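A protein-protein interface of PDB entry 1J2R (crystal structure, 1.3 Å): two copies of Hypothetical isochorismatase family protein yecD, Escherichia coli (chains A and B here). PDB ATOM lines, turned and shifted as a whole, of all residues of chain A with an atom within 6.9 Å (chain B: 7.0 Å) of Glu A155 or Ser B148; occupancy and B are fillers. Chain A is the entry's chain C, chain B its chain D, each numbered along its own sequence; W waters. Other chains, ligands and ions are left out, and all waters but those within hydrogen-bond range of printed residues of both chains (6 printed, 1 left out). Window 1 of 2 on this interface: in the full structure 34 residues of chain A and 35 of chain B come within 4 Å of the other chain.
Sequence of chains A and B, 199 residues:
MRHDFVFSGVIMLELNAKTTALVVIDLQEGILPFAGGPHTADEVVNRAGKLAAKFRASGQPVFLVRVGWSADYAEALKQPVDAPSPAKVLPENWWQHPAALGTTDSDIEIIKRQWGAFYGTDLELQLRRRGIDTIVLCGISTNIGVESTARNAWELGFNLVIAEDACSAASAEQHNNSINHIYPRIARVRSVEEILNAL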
ATOM      1  N   ARG A 128       9.989  27.529  35.408  1.00  0.00           N
ATOM      2  CA  ARG A 128       8.603  27.143  35.302  1.00  0.00           C
ATOM      3  C   ARG A 128       7.707  28.141  36.034  1.00  0.00           C
ATOM      4  O   ARG A 128       6.663  28.535  35.527  1.00  0.00           O
ATOM      5  CB  ARG A 128       8.393  25.728  35.838  1.00  0.00           C
ATOM      6  CG  ARG A 128       9.025  24.636  34.999  1.00  0.00           C
ATOM      7  CD  ARG A 128       8.433  23.278  35.328  1.00  0.00           C
ATOM      8  NE  ARG A 128       9.177  22.170  34.722  1.00  0.00           N
ATOM      9  CZ  ARG A 128       9.165  21.862  33.432  1.00  0.00           C
ATOM     10  NH1 ARG A 128       8.406  22.499  32.567  1.00  0.00           N
ATOM     11  NH2 ARG A 128       9.895  20.844  33.000  1.00  0.00           N
ATOM     12  N   ALA A 150      21.988  21.813  28.312  1.00  0.00           N
ATOM     13  CA  ALA A 150      21.138  21.760  27.132  1.00  0.00           C
ATOM     14  C   ALA A 150      20.360  20.436  27.028  1.00  0.00           C
ATOM     15  O   ALA A 150      19.160  20.427  26.738  1.00  0.00           O
ATOM     16  CB  ALA A 150      21.973  21.969  25.885  1.00  0.00           C
ATOM     17  N   ARG A 151      21.072  19.323  27.198  1.00  0.00           N
ATOM     18  CA  ARG A 151      20.450  18.014  27.117  1.00  0.00           C
ATOM     19  C   ARG A 151      19.339  17.933  28.159  1.00  0.00           C
ATOM     20  O   ARG A 151      18.234  17.490  27.864  1.00  0.00           O
ATOM     21  CB  ARG A 151      21.485  16.898  27.287  1.00  0.00           C
ATOM     22  CG  ARG A 151      22.391  16.659  26.086  1.00  0.00           C
ATOM     23  CD  ARG A 151      23.529  15.752  26.442  1.00  0.00           C
ATOM     24  NE  ARG A 151      24.508  15.525  25.381  1.00  0.00           N
ATOM     25  CZ  ARG A 151      24.583  14.441  24.607  1.00  0.00           C
ATOM     26  NH1 ARG A 151      23.718  13.449  24.712  1.00  0.00           N
ATOM     27  NH2 ARG A 151      25.546  14.368  23.699  1.00  0.00           N
ATOM     28  N   ASN A 152      19.628  18.354  29.387  1.00  0.00           N
ATOM     29  CA  ASN A 152      18.610  18.383  30.436  1.00  0.00           C
ATOM     30  C   ASN A 152      17.416  19.251  30.045  1.00  0.00           C
ATOM     31  O   ASN A 152      16.285  18.838  30.196  1.00  0.00           O
ATOM     32  CB  ASN A 152      19.130  18.977  31.756  1.00  0.00           C
ATOM     33  CG  ASN A 152      20.143  18.159  32.481  1.00  0.00           C
ATOM     34  OD1 ASN A 152      20.846  18.737  33.327  1.00  0.00           O
ATOM     35  ND2 ASN A 152      20.231  16.861  32.229  1.00  0.00           N
ATOM     36  N   ALA A 153      17.691  20.473  29.585  1.00  0.00           N
ATOM     37  CA  ALA A 153      16.638  21.447  29.311  1.00  0.00           C
ATOM     38  C   ALA A 153      15.710  20.907  28.240  1.00  0.00           C
ATOM     39  O   ALA A 153      14.496  21.060  28.325  1.00  0.00           O
ATOM     40  CB  ALA A 153      17.246  22.785  28.849  1.00  0.00           C
ATOM     41  N   TRP A 154      16.284  20.259  27.231  1.00  0.00           N
ATOM     42  CA  TRP A 154      15.477  19.716  26.142  1.00  0.00           C
ATOM     43  C   TRP A 154      14.590  18.580  26.671  1.00  0.00           C
ATOM     44  O   TRP A 154      13.417  18.509  26.338  1.00  0.00           O
ATOM     45  CB  TRP A 154      16.400  19.273  25.007  1.00  0.00           C
ATOM     46  CG  TRP A 154      15.713  18.583  23.897  1.00  0.00           C
ATOM     47  CD1 TRP A 154      14.943  19.139  22.918  1.00  0.00           C
ATOM     48  CD2 TRP A 154      15.789  17.194  23.611  1.00  0.00           C
ATOM     49  NE1 TRP A 154      14.512  18.169  22.051  1.00  0.00           N
ATOM     50  CE2 TRP A 154      15.019  16.957  22.454  1.00  0.00           C
ATOM     51  CE3 TRP A 154      16.423  16.113  24.216  1.00  0.00           C
ATOM     52  CZ2 TRP A 154      14.881  15.695  21.892  1.00  0.00           C
ATOM     53  CZ3 TRP A 154      16.265  14.832  23.647  1.00  0.00           C
ATOM     54  CH2 TRP A 154      15.504  14.655  22.501  1.00  0.00           C
ATOM     55  N   GLU A 155      15.129  17.663  27.467  1.00  0.00           N
ATOM     56  CA  GLU A 155      14.314  16.570  28.012  1.00  0.00           C
ATOM     57  C   GLU A 155      13.187  17.101  28.907  1.00  0.00           C
ATOM     58  O   GLU A 155      12.113  16.522  28.959  1.00  0.00           O
ATOM     59  CB  GLU A 155      15.169  15.546  28.753  1.00  0.00           C
ATOM     60  CG  GLU A 155      16.174  14.885  27.828  1.00  0.00           C
ATOM     61  CD  GLU A 155      16.774  13.588  28.315  1.00  0.00           C
ATOM     62  OE1 GLU A 155      16.527  13.191  29.456  1.00  0.00           O
ATOM     63  OE2 GLU A 155      17.512  12.976  27.496  1.00  0.00           O
ATOM     64  N   LEU A 156      13.435  18.216  29.584  1.00  0.00           N
ATOM     65  CA  LEU A 156      12.440  18.894  30.424  1.00  0.00           C
ATOM     66  C   LEU A 156      11.364  19.653  29.644  1.00  0.00           C
ATOM     67  O   LEU A 156      10.408  20.151  30.240  1.00  0.00           O
ATOM     68  CB  LEU A 156      13.148  19.848  31.418  1.00  0.00           C
ATOM     69  CG  LEU A 156      13.995  19.193  32.517  1.00  0.00           C
ATOM     70  CD1 LEU A 156      14.803  20.190  33.294  1.00  0.00           C
ATOM     71  CD2 LEU A 156      13.151  18.380  33.457  1.00  0.00           C
ATOM     72  N   GLY A 157      11.518  19.749  28.331  1.00  0.00           N
ATOM     73  CA  GLY A 157      10.500  20.298  27.475  1.00  0.00           C
ATOM     74  C   GLY A 157      10.719  21.736  27.071  1.00  0.00           C
ATOM     75  O   GLY A 157       9.866  22.269  26.386  1.00  0.00           O
ATOM     76  N   PHE A 158      11.814  22.366  27.477  1.00  0.00           N
ATOM     77  CA  PHE A 158      12.062  23.762  27.110  1.00  0.00           C
ATOM     78  C   PHE A 158      12.507  23.854  25.665  1.00  0.00           C
ATOM     79  O   PHE A 158      13.278  23.016  25.193  1.00  0.00           O
ATOM     80  CB  PHE A 158      13.113  24.392  28.027  1.00  0.00           C
ATOM     81  CG  PHE A 158      12.685  24.459  29.469  1.00  0.00           C
ATOM     82  CD1 PHE A 158      11.785  25.444  29.893  1.00  0.00           C
ATOM     83  CD2 PHE A 158      13.199  23.580  30.430  1.00  0.00           C
ATOM     84  CE1 PHE A 158      11.375  25.504  31.212  1.00  0.00           C
ATOM     85  CE2 PHE A 158      12.781  23.638  31.751  1.00  0.00           C
ATOM     86  CZ  PHE A 158      11.877  24.610  32.147  1.00  0.00           C
ATOM     87  N   ILE A 186      18.480  19.101  19.217  1.00  0.00           N
ATOM     88  CA  ILE A 186      17.814  19.524  20.455  1.00  0.00           C
ATOM     89  C   ILE A 186      17.525  21.018  20.563  1.00  0.00           C
ATOM     90  O   ILE A 186      16.941  21.456  21.544  1.00  0.00           O
ATOM     91  CB  ILE A 186      18.579  19.023  21.714  1.00  0.00           C
ATOM     92  CG1 ILE A 186      19.944  19.683  21.850  1.00  0.00           C
ATOM     93  CG2 ILE A 186      18.700  17.482  21.693  1.00  0.00           C
ATOM     94  CD1 ILE A 186      20.610  19.422  23.184  1.00  0.00           C
ATOM     95  N   LEU B  77       8.994  14.624  22.631  1.00  0.00           N
ATOM     96  CA  LEU B  77       9.389  16.025  22.657  1.00  0.00           C
ATOM     97  C   LEU B  77       9.152  16.661  21.289  1.00  0.00           C
ATOM     98  O   LEU B  77       9.571  16.133  20.265  1.00  0.00           O
ATOM     99  CB  LEU B  77      10.854  16.114  23.033  1.00  0.00           C
ATOM    100  CG  LEU B  77      11.134  15.717  24.488  1.00  0.00           C
ATOM    101  CD1 LEU B  77      12.625  15.422  24.725  1.00  0.00           C
ATOM    102  CD2 LEU B  77      10.639  16.800  25.432  1.00  0.00           C
ATOM    103  N   GLN B  79       9.476  20.307  20.686  1.00  0.00           N
ATOM    104  CA  GLN B  79      10.045  21.652  20.527  1.00  0.00           C
ATOM    105  C   GLN B  79      10.705  21.791  19.165  1.00  0.00           C
ATOM    106  O   GLN B  79      11.282  20.838  18.641  1.00  0.00           O
ATOM    107  CB  GLN B  79      11.149  21.936  21.554  1.00  0.00           C
ATOM    108  CG  GLN B  79      10.789  21.726  22.999  1.00  0.00           C
ATOM    109  CD  GLN B  79      11.346  20.418  23.537  1.00  0.00           C
ATOM    110  OE1 GLN B  79      12.192  20.407  24.453  1.00  0.00           O
ATOM    111  NE2 GLN B  79      10.913  19.321  22.952  1.00  0.00           N
ATOM    112  N   GLN B 114      12.914   9.664  25.226  1.00  0.00           N
ATOM    113  CA  GLN B 114      13.875  10.639  24.709  1.00  0.00           C
ATOM    114  C   GLN B 114      15.252  10.005  24.827  1.00  0.00           C
ATOM    115  O   GLN B 114      15.344   8.806  25.080  1.00  0.00           O
ATOM    116  CB  GLN B 114      13.800  11.957  25.492  1.00  0.00           C
ATOM    117  CG  GLN B 114      14.227  11.863  26.937  1.00  0.00           C
ATOM    118  CD  GLN B 114      13.228  11.130  27.820  1.00  0.00           C
ATOM    119  OE1 GLN B 114      12.030  11.429  27.812  1.00  0.00           O
ATOM    120  NE2 GLN B 114      13.721  10.199  28.631  1.00  0.00           N
ATOM    121  N   TRP B 115      16.305  10.790  24.658  1.00  0.00           N
ATOM    122  CA  TRP B 115      17.670  10.266  24.654  1.00  0.00           C
ATOM    123  C   TRP B 115      18.070   9.579  25.958  1.00  0.00           C
ATOM    124  O   TRP B 115      18.470   8.413  25.956  1.00  0.00           O
ATOM    125  CB  TRP B 115      18.664  11.383  24.321  1.00  0.00           C
ATOM    126  CG  TRP B 115      18.551  11.998  22.962  1.00  0.00           C
ATOM    127  CD1 TRP B 115      17.602  11.772  22.014  1.00  0.00           C
ATOM    128  CD2 TRP B 115      19.431  12.985  22.429  1.00  0.00           C
ATOM    129  NE1 TRP B 115      17.850  12.550  20.903  1.00  0.00           N
ATOM    130  CE2 TRP B 115      18.970  13.307  21.137  1.00  0.00           C
ATOM    131  CE3 TRP B 115      20.588  13.611  22.903  1.00  0.00           C
ATOM    132  CZ2 TRP B 115      19.639  14.204  20.316  1.00  0.00           C
ATOM    133  CZ3 TRP B 115      21.256  14.496  22.072  1.00  0.00           C
ATOM    134  CH2 TRP B 115      20.757  14.800  20.811  1.00  0.00           C
ATOM    135  N   GLY B 116      17.987  10.303  27.052  1.00  0.00           N
ATOM    136  CA  GLY B 116      18.432   9.804  28.324  1.00  0.00           C
ATOM    137  C   GLY B 116      17.465   8.803  28.937  1.00  0.00           C
ATOM    138  O   GLY B 116      16.238   8.928  28.811  1.00  0.00           O
ATOM    139  N   ALA B 117      18.014   7.826  29.648  1.00  0.00           N
ATOM    140  CA  ALA B 117      17.226   6.723  30.194  1.00  0.00           C
ATOM    141  C   ALA B 117      16.705   6.914  31.607  1.00  0.00           C
ATOM    142  O   ALA B 117      16.112   5.993  32.159  1.00  0.00           O
ATOM    143  CB  ALA B 117      18.014   5.427  30.131  1.00  0.00           C
ATOM    144  N   PHE B 118      16.917   8.095  32.187  1.00  0.00           N
ATOM    145  CA  PHE B 118      16.431   8.385  33.547  1.00  0.00           C
ATOM    146  C   PHE B 118      15.122   9.170  33.596  1.00  0.00           C
ATOM    147  O   PHE B 118      14.231   8.828  34.379  1.00  0.00           O
ATOM    148  CB  PHE B 118      17.500   9.123  34.353  1.00  0.00           C
ATOM    149  CG  PHE B 118      18.667   8.257  34.763  1.00  0.00           C
ATOM    150  CD1 PHE B 118      18.596   7.489  35.908  1.00  0.00           C
ATOM    151  CD2 PHE B 118      19.832   8.210  34.006  1.00  0.00           C
ATOM    152  CE1 PHE B 118      19.655   6.711  36.295  1.00  0.00           C
ATOM    153  CE2 PHE B 118      20.897   7.427  34.390  1.00  0.00           C
ATOM    154  CZ  PHE B 118      20.818   6.697  35.540  1.00  0.00           C
ATOM    155  N   TYR B 119      14.992  10.201  32.776  1.00  0.00           N
ATOM    156  CA  TYR B 119      13.824  11.059  32.836  1.00  0.00           C
ATOM    157  C   TYR B 119      12.579  10.271  32.453  1.00  0.00           C
ATOM    158  O   TYR B 119      12.528   9.659  31.386  1.00  0.00           O
ATOM    159  CB  TYR B 119      14.015  12.250  31.913  1.00  0.00           C
ATOM    160  CG  TYR B 119      12.881  13.250  32.029  1.00  0.00           C
ATOM    161  CD1 TYR B 119      12.797  14.117  33.120  1.00  0.00           C
ATOM    162  CD2 TYR B 119      11.883  13.295  31.069  1.00  0.00           C
ATOM    163  CE1 TYR B 119      11.729  15.045  33.212  1.00  0.00           C
ATOM    164  CE2 TYR B 119      10.837  14.214  31.156  1.00  0.00           C
ATOM    165  CZ  TYR B 119      10.782  15.073  32.217  1.00  0.00           C
ATOM    166  OH  TYR B 119       9.716  15.973  32.272  1.00  0.00           O
ATOM    167  N   GLY B 120      11.594  10.247  33.351  1.00  0.00           N
ATOM    168  CA  GLY B 120      10.350   9.552  33.103  1.00  0.00           C
ATOM    169  C   GLY B 120      10.423   8.045  33.240  1.00  0.00           C
ATOM    170  O   GLY B 120       9.485   7.352  32.836  1.00  0.00           O
ATOM    171  N   LEU B 137      27.607   0.672  31.070  1.00  0.00           N
ATOM    172  CA  LEU B 137      26.756   1.241  30.052  1.00  0.00           C
ATOM    173  C   LEU B 137      27.248   0.842  28.672  1.00  0.00           C
ATOM    174  O   LEU B 137      28.453   0.853  28.383  1.00  0.00           O
ATOM    175  CB  LEU B 137      26.781   2.755  30.206  1.00  0.00           C
ATOM    176  CG  LEU B 137      25.734   3.580  29.491  1.00  0.00           C
ATOM    177  CD1 LEU B 137      24.332   3.223  29.916  1.00  0.00           C
ATOM    178  CD2 LEU B 137      25.975   5.074  29.775  1.00  0.00           C
ATOM    179  N   SER B 141      22.915   5.267  20.566  1.00  0.00           N
ATOM    180  CA  SER B 141      24.149   5.763  19.981  1.00  0.00           C
ATOM    181  C   SER B 141      25.082   6.334  21.057  1.00  0.00           C
ATOM    182  O   SER B 141      24.641   7.042  21.982  1.00  0.00           O
ATOM    183  CB  SER B 141      23.852   6.866  18.975  1.00  0.00           C
ATOM    184  OG  SER B 141      25.046   7.506  18.625  1.00  0.00           O
ATOM    185  N   THR B 142      26.380   6.104  20.893  1.00  0.00           N
ATOM    186  CA  THR B 142      27.395   6.547  21.839  1.00  0.00           C
ATOM    187  C   THR B 142      27.222   7.981  22.332  1.00  0.00           C
ATOM    188  O   THR B 142      27.373   8.240  23.525  1.00  0.00           O
ATOM    189  CB  THR B 142      28.761   6.416  21.204  1.00  0.00           C
ATOM    190  OG1 THR B 142      28.878   5.100  20.679  1.00  0.00           O
ATOM    191  CG2 THR B 142      29.848   6.580  22.266  1.00  0.00           C
ATOM    192  N   ASN B 143      27.015   8.915  21.402  1.00  0.00           N
ATOM    193  CA  ASN B 143      26.993  10.334  21.749  1.00  0.00           C
ATOM    194  C   ASN B 143      25.590  10.894  21.869  1.00  0.00           C
ATOM    195  O   ASN B 143      25.438  12.102  22.062  1.00  0.00           O
ATOM    196  CB  ASN B 143      27.814  11.172  20.752  1.00  0.00           C
ATOM    197  CG  ASN B 143      27.205  11.196  19.352  1.00  0.00           C
ATOM    198  OD1 ASN B 143      26.639  10.209  18.895  1.00  0.00           O
ATOM    199  ND2 ASN B 143      27.322  12.330  18.663  1.00  0.00           N
ATOM    200  N   ILE B 144      24.570  10.062  21.728  1.00  0.00           N
ATOM    201  CA  ILE B 144      23.185  10.521  21.812  1.00  0.00           C
ATOM    202  C   ILE B 144      22.537   9.929  23.088  1.00  0.00           C
ATOM    203  O   ILE B 144      22.780  10.452  24.180  1.00  0.00           O
ATOM    204  CB  ILE B 144      22.418  10.210  20.476  1.00  0.00           C
ATOM    205  CG1 ILE B 144      23.223  10.709  19.254  1.00  0.00           C
ATOM    206  CG2 ILE B 144      21.049  10.843  20.480  1.00  0.00           C
ATOM    207  CD1 ILE B 144      23.429  12.219  19.176  1.00  0.00           C
ATOM    208  N   GLY B 145      21.810   8.829  22.997  1.00  0.00           N
ATOM    209  CA  GLY B 145      21.151   8.256  24.166  1.00  0.00           C
ATOM    210  C   GLY B 145      22.123   7.693  25.170  1.00  0.00           C
ATOM    211  O   GLY B 145      21.914   7.801  26.378  1.00  0.00           O
ATOM    212  N   VAL B 146      23.193   7.041  24.721  1.00  0.00           N
ATOM    213  CA  VAL B 146      24.152   6.536  25.688  1.00  0.00           C
ATOM    214  C   VAL B 146      24.744   7.699  26.505  1.00  0.00           C
ATOM    215  O   VAL B 146      24.826   7.625  27.731  1.00  0.00           O
ATOM    216  CB  VAL B 146      25.261   5.690  25.026  1.00  0.00           C
ATOM    217  CG1 VAL B 146      26.229   5.174  26.060  1.00  0.00           C
ATOM    218  CG2 VAL B 146      24.650   4.524  24.257  1.00  0.00           C
ATOM    219  N   GLU B 147      25.124   8.779  25.819  1.00  0.00           N
ATOM    220  CA  GLU B 147      25.789   9.897  26.495  1.00  0.00           C
ATOM    221  C   GLU B 147      24.856  10.686  27.416  1.00  0.00           C
ATOM    222  O   GLU B 147      25.250  11.090  28.501  1.00  0.00           O
ATOM    223  CB  GLU B 147      26.458  10.817  25.475  1.00  0.00           C
ATOM    224  CG  GLU B 147      27.345  11.843  26.130  1.00  0.00           C
ATOM    225  CD  GLU B 147      28.119  12.655  25.148  1.00  0.00           C
ATOM    226  OE1 GLU B 147      28.520  12.134  24.093  1.00  0.00           O
ATOM    227  OE2 GLU B 147      28.309  13.829  25.430  1.00  0.00           O
ATOM    228  N   SER B 148      23.611  10.894  26.998  1.00  0.00           N
ATOM    229  CA  SER B 148      22.659  11.591  27.873  1.00  0.00           C
ATOM    230  C   SER B 148      22.447  10.768  29.144  1.00  0.00           C
ATOM    231  O   SER B 148      22.402  11.306  30.242  1.00  0.00           O
ATOM    232  CB  SER B 148      21.329  11.852  27.186  1.00  0.00           C
ATOM    233  OG  SER B 148      21.440  12.929  26.253  1.00  0.00           O
ATOM    234  N   THR B 149      22.365   9.454  29.001  1.00  0.00           N
ATOM    235  CA  THR B 149      22.208   8.577  30.155  1.00  0.00           C
ATOM    236  C   THR B 149      23.440   8.654  31.050  1.00  0.00           C
ATOM    237  O   THR B 149      23.310   8.717  32.269  1.00  0.00           O
ATOM    238  CB  THR B 149      21.973   7.135  29.676  1.00  0.00           C
ATOM    239  OG1 THR B 149      20.783   7.068  28.892  1.00  0.00           O
ATOM    240  CG2 THR B 149      21.731   6.202  30.826  1.00  0.00           C
ATOM    241  N   ALA B 150      24.623   8.632  30.443  1.00  0.00           N
ATOM    242  CA  ALA B 150      25.872   8.697  31.189  1.00  0.00           C
ATOM    243  C   ALA B 150      26.024  10.002  31.970  1.00  0.00           C
ATOM    244  O   ALA B 150      26.421   9.993  33.158  1.00  0.00           O
ATOM    245  CB  ALA B 150      27.060   8.491  30.252  1.00  0.00           C
ATOM    246  N   ARG B 151      25.755  11.128  31.321  1.00  0.00           N
ATOM    247  CA  ARG B 151      25.849  12.415  31.986  1.00  0.00           C
ATOM    248  C   ARG B 151      24.902  12.456  33.193  1.00  0.00           C
ATOM    249  O   ARG B 151      25.316  12.877  34.287  1.00  0.00           O
ATOM    250  CB  ARG B 151      25.574  13.567  31.033  1.00  0.00           C
ATOM    251  CG  ARG B 151      26.646  13.785  29.975  1.00  0.00           C
ATOM    252  CD  ARG B 151      26.195  14.771  28.919  1.00  0.00           C
ATOM    253  NE  ARG B 151      27.189  15.037  27.876  1.00  0.00           N
ATOM    254  CZ  ARG B 151      27.940  16.128  27.774  1.00  0.00           C
ATOM    255  NH1 ARG B 151      27.891  17.113  28.659  1.00  0.00           N
ATOM    256  NH2 ARG B 151      28.768  16.223  26.755  1.00  0.00           N
ATOM    257  N   ASN B 152      23.665  11.993  33.015  1.00  0.00           N
ATOM    258  CA  ASN B 152      22.713  11.907  34.130  1.00  0.00           C
ATOM    259  C   ASN B 152      23.236  11.021  35.266  1.00  0.00           C
ATOM    260  O   ASN B 152      23.201  11.389  36.428  1.00  0.00           O
ATOM    261  CB  ASN B 152      21.400  11.247  33.700  1.00  0.00           C
ATOM    262  CG  ASN B 152      20.537  12.055  32.762  1.00  0.00           C
ATOM    263  OD1 ASN B 152      19.629  11.473  32.153  1.00  0.00           O
ATOM    264  ND2 ASN B 152      20.732  13.347  32.671  1.00  0.00           N
ATOM    265  N   ALA B 153      23.693   9.826  34.920  1.00  0.00           N
ATOM    266  CA  ALA B 153      24.108   8.843  35.917  1.00  0.00           C
ATOM    267  C   ALA B 153      25.227   9.394  36.771  1.00  0.00           C
ATOM    268  O   ALA B 153      25.243   9.216  37.993  1.00  0.00           O
ATOM    269  CB  ALA B 153      24.553   7.559  35.261  1.00  0.00           C
ATOM    270  N   TYR B 183      33.627  10.980  28.111  1.00  0.00           N
ATOM    271  CA  TYR B 183      33.563   9.856  29.011  1.00  0.00           C
ATOM    272  C   TYR B 183      34.725   9.740  30.000  1.00  0.00           C
ATOM    273  O   TYR B 183      34.467   9.349  31.127  1.00  0.00           O
ATOM    274  CB  TYR B 183      33.365   8.561  28.244  1.00  0.00           C
ATOM    275  CG  TYR B 183      31.993   8.408  27.639  1.00  0.00           C
ATOM    276  CD1 TYR B 183      30.866   8.463  28.422  1.00  0.00           C
ATOM    277  CD2 TYR B 183      31.812   8.178  26.287  1.00  0.00           C
ATOM    278  CE1 TYR B 183      29.617   8.282  27.878  1.00  0.00           C
ATOM    279  CE2 TYR B 183      30.559   7.984  25.737  1.00  0.00           C
ATOM    280  CZ  TYR B 183      29.452   8.065  26.544  1.00  0.00           C
ATOM    281  OH  TYR B 183      28.187   7.900  26.051  1.00  0.00           O
HETATM  282  O   HOH W   1      19.174  14.890  30.299  1.00  0.00           O
HETATM  283  O   HOH W   2      19.271  14.490  26.178  1.00  0.00           O
HETATM  284  O   HOH W   3       9.405  16.788  29.383  1.00  0.00           O
HETATM  285  O   HOH W   4      22.961  15.429  33.415  1.00  0.00           O
HETATM  286  O   HOH W   5      10.132  17.876  34.502  1.00  0.00           O
HETATM  287  O   HOH W   6      12.275  18.545  20.095  1.00  0.00           O
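The guanidinium group (NH2) of Arg A151 is in hydrogen-bond range of the backbone carbonyl oxygen (O) of Asn B143 (2.8 Å). The guanidinium group of Arg A151 sits at hydrogen-bond distance from the backbone carbonyl oxygen of Ile B144 (3.2 Å). OE2 of Glu B147 is in salt-bridge range of NH2 of Arg A151 (3.3 Å). The guanidinium group of Arg A151 is in hydrogen-bond range of the side-chain hydroxyl of Ser B148 (2.8 Å). The backbone carbonyl oxygen (O) of Trp A154 lies close to the side-chain amide oxygen (OE1) of Gln B79, 2.9 Å away. The backbone NH of Gly B116 sits at hydrogen-bond distance from the side-chain carboxylate of Glu A155, 2.8 Å away. The backbone carbonyl oxygen (O) of Phe A158 sits close to the side-chain amide oxygen (OE1) of Gln B79 (2.9 Å).
O of Ala A153 sits at hydrogen-bond distance from N of Phe A158. O of Thr B142 is in hydrogen-bond range of N of Glu B147 (3.3 Å). O of Ile B144 is in hydrogen-bond range of OG of Ser B148, 3.5 Å away. NH2 of Arg B151 lies within salt-bridge range of OE2 of Glu B147 (2.8 Å). N of Glu B147 sits close to OH of Tyr B183, 3.2 Å away. The backbone carbonyl oxygen (O) of Ser B148 sits close to the side-chain amide oxygen (OD1) of Asn B152 (3.4 Å).
Arg B151 touches Arg A151 (NE to NE, 3.7 Å). Asn B152 touches Asn A152 (ND2 to ND2, 3.6 Å). O of Trp A154 touches CD2 of Leu B77, at 3.4 Å. NE1 of Trp B115 touches CH2 of Trp A154, 3.5 Å away. Glu A155 touches Gln B114 (CD to CG, 3.4 Å). Glu A155 touches Trp B115 (OE2 to CB, 3.7 Å). Glu A155 touches Ser B148. Tyr B119 touches Leu A156. C of Gly A157 touches OE1 of Gln B79 (3.3 Å). Ile A186 touches Trp B115.
Of the printed residues of chain B, Glu A155 touches Leu B77, Gln B114, Trp B115, Gly B116, Tyr B119 and Ser B148. Of the printed residues of chain B, Ile A186 touches Trp B115 (3.5 Å). Of the printed residues of chain A, Tyr B119 touches Glu A155 (3.4 Å) and Leu A156 (3.6 Å). Of the printed residues of chain A, Ser B148 touches Arg A151 (2.8 Å) and Glu A155 (3.99 Å). The nearest printed residue of chain A that does not touch Leu B77 is Gly A157 (4.1 Å).
Printed residues of chain A that touch a printed residue of chain B: Arg A151, Asn A152, Trp A154, Glu A155, Leu A156, Gly A157, Phe A158 and Ile A186. Printed residues of chain B that touch a printed residue of chain A: Leu B77, Gln B79, Gln B114, Trp B115, Gly B116, Tyr B119, Asn B143, Ile B144, Glu B147, Ser B148, Arg B151 and Asn B152. Hydrophobic or aromatic side chains of chain B within 4 Å of the printed part of chain A: Leu B77, Trp B115 and Tyr B119. Among the printed residues, 20 pairs touch across the chains.
Arg B151 touches its own counterpart, Arg A151. Asn A152 touches its own counterpart, Asn B152.
Water W2 lies within hydrogen-bond range of OE2 of Glu A155 (2.7 Å) and OG of Ser B148 (2.7 Å). Water W3 lies within hydrogen-bond range of O of Glu A155 and OH of Tyr B119. Water W6 bridges O of Gln B79 and NE1 of Trp A154. Water W1 lies within hydrogen-bond range of the side-chain amide nitrogen (ND2) of Asn A152 (3.0 Å), the side-chain amide nitrogen (ND2) of Asn B152 (3.2 Å) and the side-chain carboxylate (OE1) of Glu A155 (3.3 Å). Water W5 lies within hydrogen-bond range of OH of Tyr B119 (3.0 Å) and NH2 of Arg A128 (3.3 Å). Water W4 bridges the side-chain amide nitrogen (ND2) of Asn B152 and the side-chain amide nitrogen (ND2) of Asn A152.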
